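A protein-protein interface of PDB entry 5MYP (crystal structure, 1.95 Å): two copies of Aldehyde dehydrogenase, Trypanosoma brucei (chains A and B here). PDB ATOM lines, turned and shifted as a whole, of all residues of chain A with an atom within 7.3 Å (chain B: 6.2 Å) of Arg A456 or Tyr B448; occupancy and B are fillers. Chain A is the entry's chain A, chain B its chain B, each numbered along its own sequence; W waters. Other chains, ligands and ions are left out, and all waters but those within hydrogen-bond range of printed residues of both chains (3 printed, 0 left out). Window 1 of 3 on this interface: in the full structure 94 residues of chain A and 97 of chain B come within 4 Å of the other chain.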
ATOM      1  N   VAL A  98       6.746 -23.065 -10.462  1.00  0.00           N
ATOM      2  CA  VAL A  98       7.992 -22.468 -10.947  1.00  0.00           C
ATOM      3  C   VAL A  98       7.670 -21.125 -11.614  1.00  0.00           C
ATOM      4  O   VAL A  98       6.655 -21.001 -12.310  1.00  0.00           O
ATOM      5  CB  VAL A  98       8.691 -23.415 -11.959  1.00  0.00           C
ATOM      6  CG1 VAL A  98       9.894 -22.753 -12.622  1.00  0.00           C
ATOM      7  CG2 VAL A  98       9.110 -24.709 -11.272  1.00  0.00           C
ATOM      8  N   LYS A  99       8.531 -20.131 -11.392  1.00  0.00           N
ATOM      9  CA  LYS A  99       8.401 -18.820 -12.020  1.00  0.00           C
ATOM     10  C   LYS A  99       9.244 -18.795 -13.301  1.00  0.00           C
ATOM     11  O   LYS A  99      10.473 -18.723 -13.222  1.00  0.00           O
ATOM     12  CB  LYS A  99       8.854 -17.710 -11.058  1.00  0.00           C
ATOM     13  CG  LYS A  99       8.090 -17.648  -9.740  1.00  0.00           C
ATOM     14  CD  LYS A  99       6.644 -17.194  -9.893  1.00  0.00           C
ATOM     15  CE  LYS A  99       6.521 -15.689 -10.068  1.00  0.00           C
ATOM     16  NZ  LYS A  99       5.164 -15.310 -10.570  1.00  0.00           N
ATOM     17  N   PRO A 100       8.600 -18.869 -14.483  1.00  0.00           N
ATOM     18  CA  PRO A 100       9.368 -18.908 -15.728  1.00  0.00           C
ATOM     19  C   PRO A 100      10.003 -17.566 -16.097  1.00  0.00           C
ATOM     20  O   PRO A 100       9.532 -16.516 -15.668  1.00  0.00           O
ATOM     21  CB  PRO A 100       8.316 -19.279 -16.771  1.00  0.00           C
ATOM     22  CG  PRO A 100       7.069 -18.663 -16.254  1.00  0.00           C
ATOM     23  CD  PRO A 100       7.155 -18.787 -14.755  1.00  0.00           C
ATOM     24  N   THR A 101      11.060 -17.630 -16.900  1.00  0.00           N
ATOM     25  CA  THR A 101      11.721 -16.442 -17.433  1.00  0.00           C
ATOM     26  C   THR A 101      10.862 -15.867 -18.557  1.00  0.00           C
ATOM     27  O   THR A 101      10.681 -16.517 -19.598  1.00  0.00           O
ATOM     28  CB  THR A 101      13.128 -16.783 -17.968  1.00  0.00           C
ATOM     29  OG1 THR A 101      13.914 -17.335 -16.907  1.00  0.00           O
ATOM     30  CG2 THR A 101      13.826 -15.538 -18.529  1.00  0.00           C
ATOM     31  N   MET A 102      10.329 -14.663 -18.332  1.00  0.00           N
ATOM     32  CA  MET A 102       9.435 -14.005 -19.282  1.00  0.00           C
ATOM     33  C   MET A 102      10.142 -12.893 -20.050  1.00  0.00           C
ATOM     34  O   MET A 102      10.978 -12.188 -19.494  1.00  0.00           O
ATOM     35  CB  MET A 102       8.211 -13.450 -18.552  1.00  0.00           C
ATOM     36  CG  MET A 102       7.381 -14.488 -17.791  1.00  0.00           C
ATOM     37  SD  MET A 102       6.854 -15.901 -18.787  1.00  0.00           S
ATOM     38  CE  MET A 102       5.834 -15.120 -20.039  1.00  0.00           C
ATOM     39  N   GLU A 112       3.216 -18.279 -13.963  1.00  0.00           N
ATOM     40  CA  GLU A 112       3.640 -19.452 -13.188  1.00  0.00           C
ATOM     41  C   GLU A 112       3.521 -20.724 -14.021  1.00  0.00           C
ATOM     42  O   GLU A 112       2.668 -20.801 -14.906  1.00  0.00           O
ATOM     43  CB  GLU A 112       2.725 -19.648 -11.977  1.00  0.00           C
ATOM     44  CG  GLU A 112       3.021 -18.788 -10.768  1.00  0.00           C
ATOM     45  CD  GLU A 112       2.146 -19.178  -9.574  1.00  0.00           C
ATOM     46  OE1 GLU A 112       1.210 -19.999  -9.725  1.00  0.00           O
ATOM     47  OE2 GLU A 112       2.384 -18.658  -8.471  1.00  0.00           O
ATOM     48  N   LEU A 113       4.366 -21.709 -13.723  1.00  0.00           N
ATOM     49  CA  LEU A 113       4.212 -23.069 -14.243  1.00  0.00           C
ATOM     50  C   LEU A 113       3.834 -23.967 -13.068  1.00  0.00           C
ATOM     51  O   LEU A 113       4.656 -24.220 -12.186  1.00  0.00           O
ATOM     52  CB  LEU A 113       5.503 -23.553 -14.908  1.00  0.00           C
ATOM     53  CG  LEU A 113       6.104 -22.637 -15.980  1.00  0.00           C
ATOM     54  CD1 LEU A 113       7.360 -23.268 -16.566  1.00  0.00           C
ATOM     55  CD2 LEU A 113       5.101 -22.312 -17.073  1.00  0.00           C
ATOM     56  N   GLN A 114       2.576 -24.401 -13.030  1.00  0.00           N
ATOM     57  CA  GLN A 114       2.070 -25.278 -11.968  1.00  0.00           C
ATOM     58  C   GLN A 114       2.156 -26.723 -12.438  1.00  0.00           C
ATOM     59  O   GLN A 114       2.161 -26.984 -13.641  1.00  0.00           O
ATOM     60  CB  GLN A 114       0.619 -24.928 -11.614  1.00  0.00           C
ATOM     61  CG  GLN A 114       0.418 -23.511 -11.074  1.00  0.00           C
ATOM     62  CD  GLN A 114      -1.031 -23.192 -10.733  1.00  0.00           C
ATOM     63  OE1 GLN A 114      -1.929 -24.025 -10.899  1.00  0.00           O
ATOM     64  NE2 GLN A 114      -1.268 -21.971 -10.252  1.00  0.00           N
ATOM     65  N   TYR A 115       2.234 -27.658 -11.496  1.00  0.00           N
ATOM     66  CA  TYR A 115       2.223 -29.089 -11.804  1.00  0.00           C
ATOM     67  C   TYR A 115       0.948 -29.698 -11.267  1.00  0.00           C
ATOM     68  O   TYR A 115       0.595 -29.462 -10.116  1.00  0.00           O
ATOM     69  CB  TYR A 115       3.443 -29.781 -11.198  1.00  0.00           C
ATOM     70  CG  TYR A 115       4.723 -29.322 -11.833  1.00  0.00           C
ATOM     71  CD1 TYR A 115       5.219 -29.954 -12.970  1.00  0.00           C
ATOM     72  CD2 TYR A 115       5.422 -28.224 -11.327  1.00  0.00           C
ATOM     73  CE1 TYR A 115       6.394 -29.527 -13.574  1.00  0.00           C
ATOM     74  CE2 TYR A 115       6.598 -27.788 -11.923  1.00  0.00           C
ATOM     75  CZ  TYR A 115       7.079 -28.445 -13.041  1.00  0.00           C
ATOM     76  OH  TYR A 115       8.245 -28.016 -13.623  1.00  0.00           O
ATOM     77  N   GLU A 116       0.250 -30.471 -12.102  1.00  0.00           N
ATOM     78  CA  GLU A 116      -0.976 -31.153 -11.687  1.00  0.00           C
ATOM     79  C   GLU A 116      -0.929 -32.640 -12.049  1.00  0.00           C
ATOM     80  O   GLU A 116      -0.245 -33.023 -13.008  1.00  0.00           O
ATOM     81  CB  GLU A 116      -2.217 -30.489 -12.308  1.00  0.00           C
ATOM     82  CG  GLU A 116      -2.266 -30.502 -13.830  1.00  0.00           C
ATOM     83  CD  GLU A 116      -3.586 -30.013 -14.411  1.00  0.00           C
ATOM     84  OE1 GLU A 116      -4.499 -29.627 -13.652  1.00  0.00           O
ATOM     85  OE2 GLU A 116      -3.719 -30.024 -15.654  1.00  0.00           O
ATOM     86  N   LEU A 118      -2.151 -36.264 -13.638  1.00  0.00           N
ATOM     87  CA  LEU A 118      -2.743 -36.636 -14.926  1.00  0.00           C
ATOM     88  C   LEU A 118      -4.061 -37.404 -14.773  1.00  0.00           C
ATOM     89  O   LEU A 118      -5.028 -37.125 -15.477  1.00  0.00           O
ATOM     90  CB  LEU A 118      -1.754 -37.478 -15.736  1.00  0.00           C
ATOM     91  CG  LEU A 118      -0.497 -36.745 -16.201  1.00  0.00           C
ATOM     92  CD1 LEU A 118       0.524 -37.738 -16.740  1.00  0.00           C
ATOM     93  CD2 LEU A 118      -0.824 -35.679 -17.238  1.00  0.00           C
ATOM     94  N   GLU A 451       7.869 -35.325 -13.000  1.00  0.00           N
ATOM     95  CA  GLU A 451       7.574 -34.544 -14.203  1.00  0.00           C
ATOM     96  C   GLU A 451       6.832 -35.364 -15.262  1.00  0.00           C
ATOM     97  O   GLU A 451       5.841 -34.897 -15.814  1.00  0.00           O
ATOM     98  CB  GLU A 451       8.854 -33.938 -14.786  1.00  0.00           C
ATOM     99  CG  GLU A 451       9.425 -32.825 -13.923  1.00  0.00           C
ATOM    100  CD  GLU A 451      10.783 -32.331 -14.396  1.00  0.00           C
ATOM    101  OE1 GLU A 451      11.320 -32.849 -15.402  1.00  0.00           O
ATOM    102  OE2 GLU A 451      11.314 -31.406 -13.756  1.00  0.00           O
ATOM    103  N   SER A 454       3.129 -35.904 -14.371  1.00  0.00           N
ATOM    104  CA  SER A 454       2.402 -34.667 -14.105  1.00  0.00           C
ATOM    105  C   SER A 454       2.182 -33.902 -15.403  1.00  0.00           C
ATOM    106  O   SER A 454       2.869 -34.138 -16.401  1.00  0.00           O
ATOM    107  CB  SER A 454       3.200 -33.756 -13.154  1.00  0.00           C
ATOM    108  OG  SER A 454       3.389 -34.345 -11.889  1.00  0.00           O
ATOM    109  N   HIS A 455       1.226 -32.985 -15.373  1.00  0.00           N
ATOM    110  CA  HIS A 455       1.052 -32.017 -16.431  1.00  0.00           C
ATOM    111  C   HIS A 455       1.599 -30.678 -15.945  1.00  0.00           C
ATOM    112  O   HIS A 455       1.144 -30.157 -14.928  1.00  0.00           O
ATOM    113  CB  HIS A 455      -0.419 -31.880 -16.820  1.00  0.00           C
ATOM    114  CG  HIS A 455      -0.670 -30.766 -17.780  1.00  0.00           C
ATOM    115  ND1 HIS A 455       0.180 -30.509 -18.828  1.00  0.00           N
ATOM    116  CD2 HIS A 455      -1.661 -29.849 -17.863  1.00  0.00           C
ATOM    117  CE1 HIS A 455      -0.277 -29.483 -19.518  1.00  0.00           C
ATOM    118  NE2 HIS A 455      -1.391 -29.060 -18.953  1.00  0.00           N
ATOM    119  N   ARG A 456       2.578 -30.138 -16.666  1.00  0.00           N
ATOM    120  CA  ARG A 456       3.093 -28.793 -16.398  1.00  0.00           C
ATOM    121  C   ARG A 456       2.131 -27.790 -17.034  1.00  0.00           C
ATOM    122  O   ARG A 456       2.015 -27.729 -18.257  1.00  0.00           O
ATOM    123  CB  ARG A 456       4.509 -28.635 -16.962  1.00  0.00           C
ATOM    124  CG  ARG A 456       5.154 -27.292 -16.656  1.00  0.00           C
ATOM    125  CD  ARG A 456       6.581 -27.225 -17.157  1.00  0.00           C
ATOM    126  NE  ARG A 456       6.685 -27.534 -18.579  1.00  0.00           N
ATOM    127  CZ  ARG A 456       7.830 -27.698 -19.238  1.00  0.00           C
ATOM    128  NH1 ARG A 456       9.006 -27.557 -18.625  1.00  0.00           N
ATOM    129  NH2 ARG A 456       7.804 -27.991 -20.533  1.00  0.00           N
ATOM    130  N   ARG A 457       1.451 -27.013 -16.196  1.00  0.00           N
ATOM    131  CA  ARG A 457       0.338 -26.164 -16.604  1.00  0.00           C
ATOM    132  C   ARG A 457       0.665 -24.679 -16.437  1.00  0.00           C
ATOM    133  O   ARG A 457       0.730 -24.195 -15.305  1.00  0.00           O
ATOM    134  CB  ARG A 457      -0.891 -26.522 -15.771  1.00  0.00           C
ATOM    135  CG  ARG A 457      -2.190 -25.876 -16.227  1.00  0.00           C
ATOM    136  CD  ARG A 457      -3.253 -26.148 -15.187  1.00  0.00           C
ATOM    137  NE  ARG A 457      -4.630 -25.888 -15.618  1.00  0.00           N
ATOM    138  CZ  ARG A 457      -5.669 -25.811 -14.785  1.00  0.00           C
ATOM    139  NH1 ARG A 457      -5.503 -25.954 -13.465  1.00  0.00           N
ATOM    140  NH2 ARG A 457      -6.889 -25.574 -15.263  1.00  0.00           N
ATOM    141  N   PRO A 458       0.869 -23.950 -17.552  1.00  0.00           N
ATOM    142  CA  PRO A 458       1.162 -22.519 -17.445  1.00  0.00           C
ATOM    143  C   PRO A 458      -0.046 -21.697 -17.001  1.00  0.00           C
ATOM    144  O   PRO A 458      -1.166 -21.960 -17.443  1.00  0.00           O
ATOM    145  CB  PRO A 458       1.570 -22.134 -18.874  1.00  0.00           C
ATOM    146  CG  PRO A 458       0.879 -23.129 -19.732  1.00  0.00           C
ATOM    147  CD  PRO A 458       0.945 -24.406 -18.952  1.00  0.00           C
ATOM    148  N   TYR B  94      20.769 -22.444 -24.871  1.00  0.00           N
ATOM    149  CA  TYR B  94      20.001 -23.698 -24.918  1.00  0.00           C
ATOM    150  C   TYR B  94      20.849 -24.932 -25.242  1.00  0.00           C
ATOM    151  O   TYR B  94      20.600 -26.006 -24.698  1.00  0.00           O
ATOM    152  CB  TYR B  94      18.822 -23.585 -25.904  1.00  0.00           C
ATOM    153  CG  TYR B  94      17.769 -22.530 -25.563  1.00  0.00           C
ATOM    154  CD1 TYR B  94      17.633 -22.009 -24.265  1.00  0.00           C
ATOM    155  CD2 TYR B  94      16.877 -22.080 -26.539  1.00  0.00           C
ATOM    156  CE1 TYR B  94      16.667 -21.061 -23.970  1.00  0.00           C
ATOM    157  CE2 TYR B  94      15.902 -21.133 -26.245  1.00  0.00           C
ATOM    158  CZ  TYR B  94      15.802 -20.631 -24.958  1.00  0.00           C
ATOM    159  OH  TYR B  94      14.861 -19.690 -24.627  1.00  0.00           O
ATOM    160  N   SER B 414      -6.450 -28.038 -17.590  1.00  0.00           N
ATOM    161  CA  SER B 414      -6.476 -27.449 -18.920  1.00  0.00           C
ATOM    162  C   SER B 414      -5.050 -27.267 -19.407  1.00  0.00           C
ATOM    163  O   SER B 414      -4.117 -27.351 -18.612  1.00  0.00           O
ATOM    164  CB  SER B 414      -7.188 -26.095 -18.884  1.00  0.00           C
ATOM    165  OG  SER B 414      -6.569 -25.220 -17.953  1.00  0.00           O
ATOM    166  N   GLY B 415      -4.885 -27.016 -20.702  1.00  0.00           N
ATOM    167  CA  GLY B 415      -3.565 -26.755 -21.277  1.00  0.00           C
ATOM    168  C   GLY B 415      -2.918 -25.495 -20.713  1.00  0.00           C
ATOM    169  O   GLY B 415      -1.696 -25.417 -20.620  1.00  0.00           O
ATOM    170  N   GLY B 430       8.033 -17.201 -22.915  1.00  0.00           N
ATOM    171  CA  GLY B 430       8.399 -17.781 -21.623  1.00  0.00           C
ATOM    172  C   GLY B 430       7.471 -18.875 -21.126  1.00  0.00           C
ATOM    173  O   GLY B 430       7.823 -19.593 -20.193  1.00  0.00           O
ATOM    174  N   LEU B 431       6.283 -18.998 -21.726  1.00  0.00           N
ATOM    175  CA  LEU B 431       5.345 -20.072 -21.391  1.00  0.00           C
ATOM    176  C   LEU B 431       5.426 -21.195 -22.428  1.00  0.00           C
ATOM    177  O   LEU B 431       5.515 -20.917 -23.632  1.00  0.00           O
ATOM    178  CB  LEU B 431       3.913 -19.547 -21.347  1.00  0.00           C
ATOM    179  CG  LEU B 431       3.575 -18.467 -20.315  1.00  0.00           C
ATOM    180  CD1 LEU B 431       2.100 -18.114 -20.398  1.00  0.00           C
ATOM    181  CD2 LEU B 431       3.941 -18.912 -18.906  1.00  0.00           C
ATOM    182  N   PRO B 432       5.391 -22.467 -21.972  1.00  0.00           N
ATOM    183  CA  PRO B 432       5.210 -23.575 -22.910  1.00  0.00           C
ATOM    184  C   PRO B 432       3.764 -23.609 -23.392  1.00  0.00           C
ATOM    185  O   PRO B 432       2.849 -23.392 -22.590  1.00  0.00           O
ATOM    186  CB  PRO B 432       5.537 -24.818 -22.068  1.00  0.00           C
ATOM    187  CG  PRO B 432       5.260 -24.419 -20.663  1.00  0.00           C
ATOM    188  CD  PRO B 432       5.443 -22.928 -20.571  1.00  0.00           C
ATOM    189  N   PHE B 433       3.559 -23.864 -24.683  1.00  0.00           N
ATOM    190  CA  PHE B 433       2.219 -23.911 -25.255  1.00  0.00           C
ATOM    191  C   PHE B 433       1.859 -25.334 -25.651  1.00  0.00           C
ATOM    192  O   PHE B 433       2.498 -25.917 -26.520  1.00  0.00           O
ATOM    193  CB  PHE B 433       2.099 -22.992 -26.469  1.00  0.00           C
ATOM    194  CG  PHE B 433       0.699 -22.901 -27.000  1.00  0.00           C
ATOM    195  CD1 PHE B 433      -0.228 -22.056 -26.399  1.00  0.00           C
ATOM    196  CD2 PHE B 433       0.293 -23.684 -28.073  1.00  0.00           C
ATOM    197  CE1 PHE B 433      -1.528 -21.982 -26.865  1.00  0.00           C
ATOM    198  CE2 PHE B 433      -1.012 -23.611 -28.549  1.00  0.00           C
ATOM    199  CZ  PHE B 433      -1.923 -22.761 -27.941  1.00  0.00           C
ATOM    200  N   ALA B 443       4.461 -29.862 -25.627  1.00  0.00           N
ATOM    201  CA  ALA B 443       4.383 -28.407 -25.681  1.00  0.00           C
ATOM    202  C   ALA B 443       5.587 -27.846 -26.416  1.00  0.00           C
ATOM    203  O   ALA B 443       6.628 -28.498 -26.495  1.00  0.00           O
ATOM    204  CB  ALA B 443       4.299 -27.829 -24.279  1.00  0.00           C
ATOM    205  N   TYR B 444       5.431 -26.649 -26.968  1.00  0.00           N
ATOM    206  CA  TYR B 444       6.525 -25.974 -27.672  1.00  0.00           C
ATOM    207  C   TYR B 444       6.432 -24.444 -27.494  1.00  0.00           C
ATOM    208  O   TYR B 444       5.674 -23.978 -26.639  1.00  0.00           O
ATOM    209  CB  TYR B 444       6.574 -26.447 -29.141  1.00  0.00           C
ATOM    210  CG  TYR B 444       5.533 -25.875 -30.080  1.00  0.00           C
ATOM    211  CD1 TYR B 444       4.177 -26.159 -29.908  1.00  0.00           C
ATOM    212  CD2 TYR B 444       5.903 -25.087 -31.175  1.00  0.00           C
ATOM    213  CE1 TYR B 444       3.220 -25.654 -30.780  1.00  0.00           C
ATOM    214  CE2 TYR B 444       4.952 -24.582 -32.050  1.00  0.00           C
ATOM    215  CZ  TYR B 444       3.615 -24.868 -31.851  1.00  0.00           C
ATOM    216  OH  TYR B 444       2.668 -24.365 -32.717  1.00  0.00           O
ATOM    217  N   HIS B 445       7.217 -23.705 -28.285  1.00  0.00           N
ATOM    218  CA  HIS B 445       7.452 -22.241 -28.201  1.00  0.00           C
ATOM    219  C   HIS B 445       8.771 -22.010 -27.475  1.00  0.00           C
ATOM    220  O   HIS B 445       8.946 -22.480 -26.353  1.00  0.00           O
ATOM    221  CB  HIS B 445       6.335 -21.418 -27.526  1.00  0.00           C
ATOM    222  CG  HIS B 445       5.039 -21.411 -28.273  1.00  0.00           C
ATOM    223  ND1 HIS B 445       4.037 -20.497 -28.018  1.00  0.00           N
ATOM    224  CD2 HIS B 445       4.587 -22.194 -29.283  1.00  0.00           C
ATOM    225  CE1 HIS B 445       3.020 -20.730 -28.831  1.00  0.00           C
ATOM    226  NE2 HIS B 445       3.329 -21.753 -29.606  1.00  0.00           N
ATOM    227  N   GLY B 446       9.703 -21.323 -28.145  1.00  0.00           N
ATOM    228  CA  GLY B 446      10.956 -20.870 -27.533  1.00  0.00           C
ATOM    229  C   GLY B 446      11.826 -21.996 -27.009  1.00  0.00           C
ATOM    230  O   GLY B 446      12.101 -22.954 -27.731  1.00  0.00           O
ATOM    231  N   ARG B 447      12.244 -21.883 -25.747  1.00  0.00           N
ATOM    232  CA  ARG B 447      12.995 -22.943 -25.051  1.00  0.00           C
ATOM    233  C   ARG B 447      12.308 -24.314 -25.110  1.00  0.00           C
ATOM    234  O   ARG B 447      12.978 -25.345 -25.194  1.00  0.00           O
ATOM    235  CB  ARG B 447      13.198 -22.570 -23.576  1.00  0.00           C
ATOM    236  CG  ARG B 447      14.144 -23.489 -22.814  1.00  0.00           C
ATOM    237  CD  ARG B 447      14.639 -22.842 -21.522  1.00  0.00           C
ATOM    238  NE  ARG B 447      15.983 -23.312 -21.168  1.00  0.00           N
ATOM    239  CZ  ARG B 447      16.903 -22.604 -20.507  1.00  0.00           C
ATOM    240  NH1 ARG B 447      16.670 -21.359 -20.087  1.00  0.00           N
ATOM    241  NH2 ARG B 447      18.089 -23.153 -20.257  1.00  0.00           N
ATOM    242  N   TYR B 448      10.978 -24.310 -25.059  1.00  0.00           N
ATOM    243  CA  TYR B 448      10.200 -25.549 -24.998  1.00  0.00           C
ATOM    244  C   TYR B 448      10.134 -26.242 -26.367  1.00  0.00           C
ATOM    245  O   TYR B 448      10.027 -27.466 -26.433  1.00  0.00           O
ATOM    246  CB  TYR B 448       8.816 -25.273 -24.402  1.00  0.00           C
ATOM    247  CG  TYR B 448       8.945 -24.568 -23.069  1.00  0.00           C
ATOM    248  CD1 TYR B 448       9.367 -25.262 -21.938  1.00  0.00           C
ATOM    249  CD2 TYR B 448       8.704 -23.196 -22.947  1.00  0.00           C
ATOM    250  CE1 TYR B 448       9.525 -24.620 -20.717  1.00  0.00           C
ATOM    251  CE2 TYR B 448       8.856 -22.547 -21.723  1.00  0.00           C
ATOM    252  CZ  TYR B 448       9.266 -23.268 -20.616  1.00  0.00           C
ATOM    253  OH  TYR B 448       9.420 -22.656 -19.396  1.00  0.00           O
ATOM    254  N   SER B 449      10.219 -25.458 -27.446  1.00  0.00           N
ATOM    255  CA  SER B 449      10.450 -26.016 -28.781  1.00  0.00           C
ATOM    256  C   SER B 449      11.814 -26.687 -28.837  1.00  0.00           C
ATOM    257  O   SER B 449      11.930 -27.825 -29.286  1.00  0.00           O
ATOM    258  CB  SER B 449      10.387 -24.947 -29.872  1.00  0.00           C
ATOM    259  OG  SER B 449       9.071 -24.477 -30.075  1.00  0.00           O
ATOM    260  N   PHE B 450      12.846 -25.986 -28.372  1.00  0.00           N
ATOM    261  CA  PHE B 450      14.190 -26.545 -28.378  1.00  0.00           C
ATOM    262  C   PHE B 450      14.228 -27.879 -27.624  1.00  0.00           C
ATOM    263  O   PHE B 450      14.777 -28.862 -28.126  1.00  0.00           O
ATOM    264  CB  PHE B 450      15.222 -25.573 -27.792  1.00  0.00           C
ATOM    265  CG  PHE B 450      16.615 -26.111 -27.824  1.00  0.00           C
ATOM    266  CD1 PHE B 450      17.098 -26.881 -26.771  1.00  0.00           C
ATOM    267  CD2 PHE B 450      17.426 -25.907 -28.932  1.00  0.00           C
ATOM    268  CE1 PHE B 450      18.379 -27.409 -26.812  1.00  0.00           C
ATOM    269  CE2 PHE B 450      18.709 -26.439 -28.975  1.00  0.00           C
ATOM    270  CZ  PHE B 450      19.184 -27.189 -27.919  1.00  0.00           C
ATOM    271  N   GLU B 451      13.626 -27.904 -26.438  1.00  0.00           N
ATOM    272  CA  GLU B 451      13.567 -29.121 -25.623  1.00  0.00           C
ATOM    273  C   GLU B 451      12.762 -30.237 -26.300  1.00  0.00           C
ATOM    274  O   GLU B 451      13.213 -31.372 -26.352  1.00  0.00           O
ATOM    275  CB  GLU B 451      13.023 -28.812 -24.226  1.00  0.00           C
ATOM    276  CG  GLU B 451      14.021 -28.014 -23.393  1.00  0.00           C
ATOM    277  CD  GLU B 451      13.487 -27.538 -22.052  1.00  0.00           C
ATOM    278  OE1 GLU B 451      14.236 -26.817 -21.365  1.00  0.00           O
ATOM    279  OE2 GLU B 451      12.342 -27.868 -21.673  1.00  0.00           O
ATOM    280  N   THR B 452      11.596 -29.891 -26.836  1.00  0.00           N
ATOM    281  CA  THR B 452      10.726 -30.861 -27.525  1.00  0.00           C
ATOM    282  C   THR B 452      11.407 -31.521 -28.731  1.00  0.00           C
ATOM    283  O   THR B 452      11.246 -32.714 -28.943  1.00  0.00           O
ATOM    284  CB  THR B 452       9.399 -30.203 -27.949  1.00  0.00           C
ATOM    285  OG1 THR B 452       8.659 -29.883 -26.770  1.00  0.00           O
ATOM    286  CG2 THR B 452       8.544 -31.121 -28.835  1.00  0.00           C
ATOM    287  N   PHE B 453      12.179 -30.745 -29.493  1.00  0.00           N
ATOM    288  CA  PHE B 453      12.860 -31.256 -30.692  1.00  0.00           C
ATOM    289  C   PHE B 453      14.319 -31.684 -30.458  1.00  0.00           C
ATOM    290  O   PHE B 453      15.086 -31.836 -31.415  1.00  0.00           O
ATOM    291  CB  PHE B 453      12.748 -30.221 -31.817  1.00  0.00           C
ATOM    292  CG  PHE B 453      11.324 -29.883 -32.186  1.00  0.00           C
ATOM    293  CD1 PHE B 453      10.465 -30.874 -32.648  1.00  0.00           C
ATOM    294  CD2 PHE B 453      10.849 -28.576 -32.100  1.00  0.00           C
ATOM    295  CE1 PHE B 453       9.157 -30.575 -32.999  1.00  0.00           C
ATOM    296  CE2 PHE B 453       9.545 -28.270 -32.449  1.00  0.00           C
ATOM    297  CZ  PHE B 453       8.696 -29.274 -32.897  1.00  0.00           C
HETATM  298  O   HOH W   1      10.069 -28.910 -22.113  1.00  0.00           O
HETATM  299  O   HOH W   2       0.140 -27.244 -21.291  1.00  0.00           O
HETATM  300  O   HOH W   3      11.330 -16.416 -22.288  1.00  0.00           O
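N of Leu A113 lies within hydrogen-bond range of O of Val A98. O of Gln A114 is in hydrogen-bond range of N of Arg A457. The backbone carbonyl oxygen of Glu A116 is in hydrogen-bond range of the backbone NH of His A455, at 2.8 Å. The guanidinium group (NH1) of Arg A457 is in salt-bridge range of the side-chain carboxylate (OE1) of Glu A116. The backbone carbonyl oxygen (O) of Tyr B448 sits at hydrogen-bond distance from the side-chain hydroxyl (OG1) of Thr B452, at 2.8 Å.
1 position is printed for both chains. Of the 12 pairs that touch across the chains among the printed residues, none has its exchanged pair printed and touching as well.
Pro A100 touches Gly B430 (CB to O, 3.5 Å). CA of Gly B430 touches O of Thr A101, 3.3 Å away. Met A102 touches Gly B430. Leu A113 touches Pro B432. Leu A113 touches Tyr B448. N of Ser B414 touches OE2 of Glu A116 (3.9 Å). His A455 touches Gly B415 (NE2 to CA, 3.9 Å). Tyr B448 touches Arg A456. Pro A458 touches Gly B415 (CD to O, 3.3 Å). CG of Pro A458 touches O of Pro B432, 3.5 Å away.
Of the printed residues of chain B, Arg A456 touches Tyr B448 (3.4 Å). Of the printed residues of chain B, Pro A458 touches Gly B415 (3.3 Å) and Pro B432 (3.5 Å). Printed residues of chain A within 4 Å of Ser B414: Glu A116, His A455 and Arg A457. Printed residues of chain A within 4 Å of Gly B415: His A455 (3.9 Å) and Pro A458 (3.3 Å). Printed residues of chain A within 4 Å of Pro B432: Leu A113 and Pro A458. Of chain A, only Leu A113 (3.6 Å) and Arg A456 (3.4 Å) come within 4 Å of Tyr B448. The nearest printed residue of chain A that does not touch Pro B432 is Arg A456 (4.01 Å).
NE2 of His A455 lies within hydrogen-bond range of O of Ser B414 (3.2 Å). NH2 of Arg A457 is in hydrogen-bond range of OG of Ser B414 (2.7 Å).
Of the 17 printed residues of chain A, 9 touch a printed residue of chain B. Hydrophobic or aromatic side chains of chain A within 4 Å of the printed part of chain B: Pro A100, Met A102, Leu A113, His A455 and Pro A458. Hydrophobic or aromatic side chains of chain B that line the printed part of chain A: Pro B432 and Tyr B448. Among the printed residues, 12 pairs touch across the chains.
Water W1 bridges the side-chain carboxylate of Glu B451 (2.5 Å) and the guanidinium group of Arg A456 (2.9 Å). Water W2 bridges O of Gly B415 (2.7 Å) and NE2 of His A455 (3.3 Å). Water W3 lies within hydrogen-bond range of O of Thr A101 and N of Gly B430.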
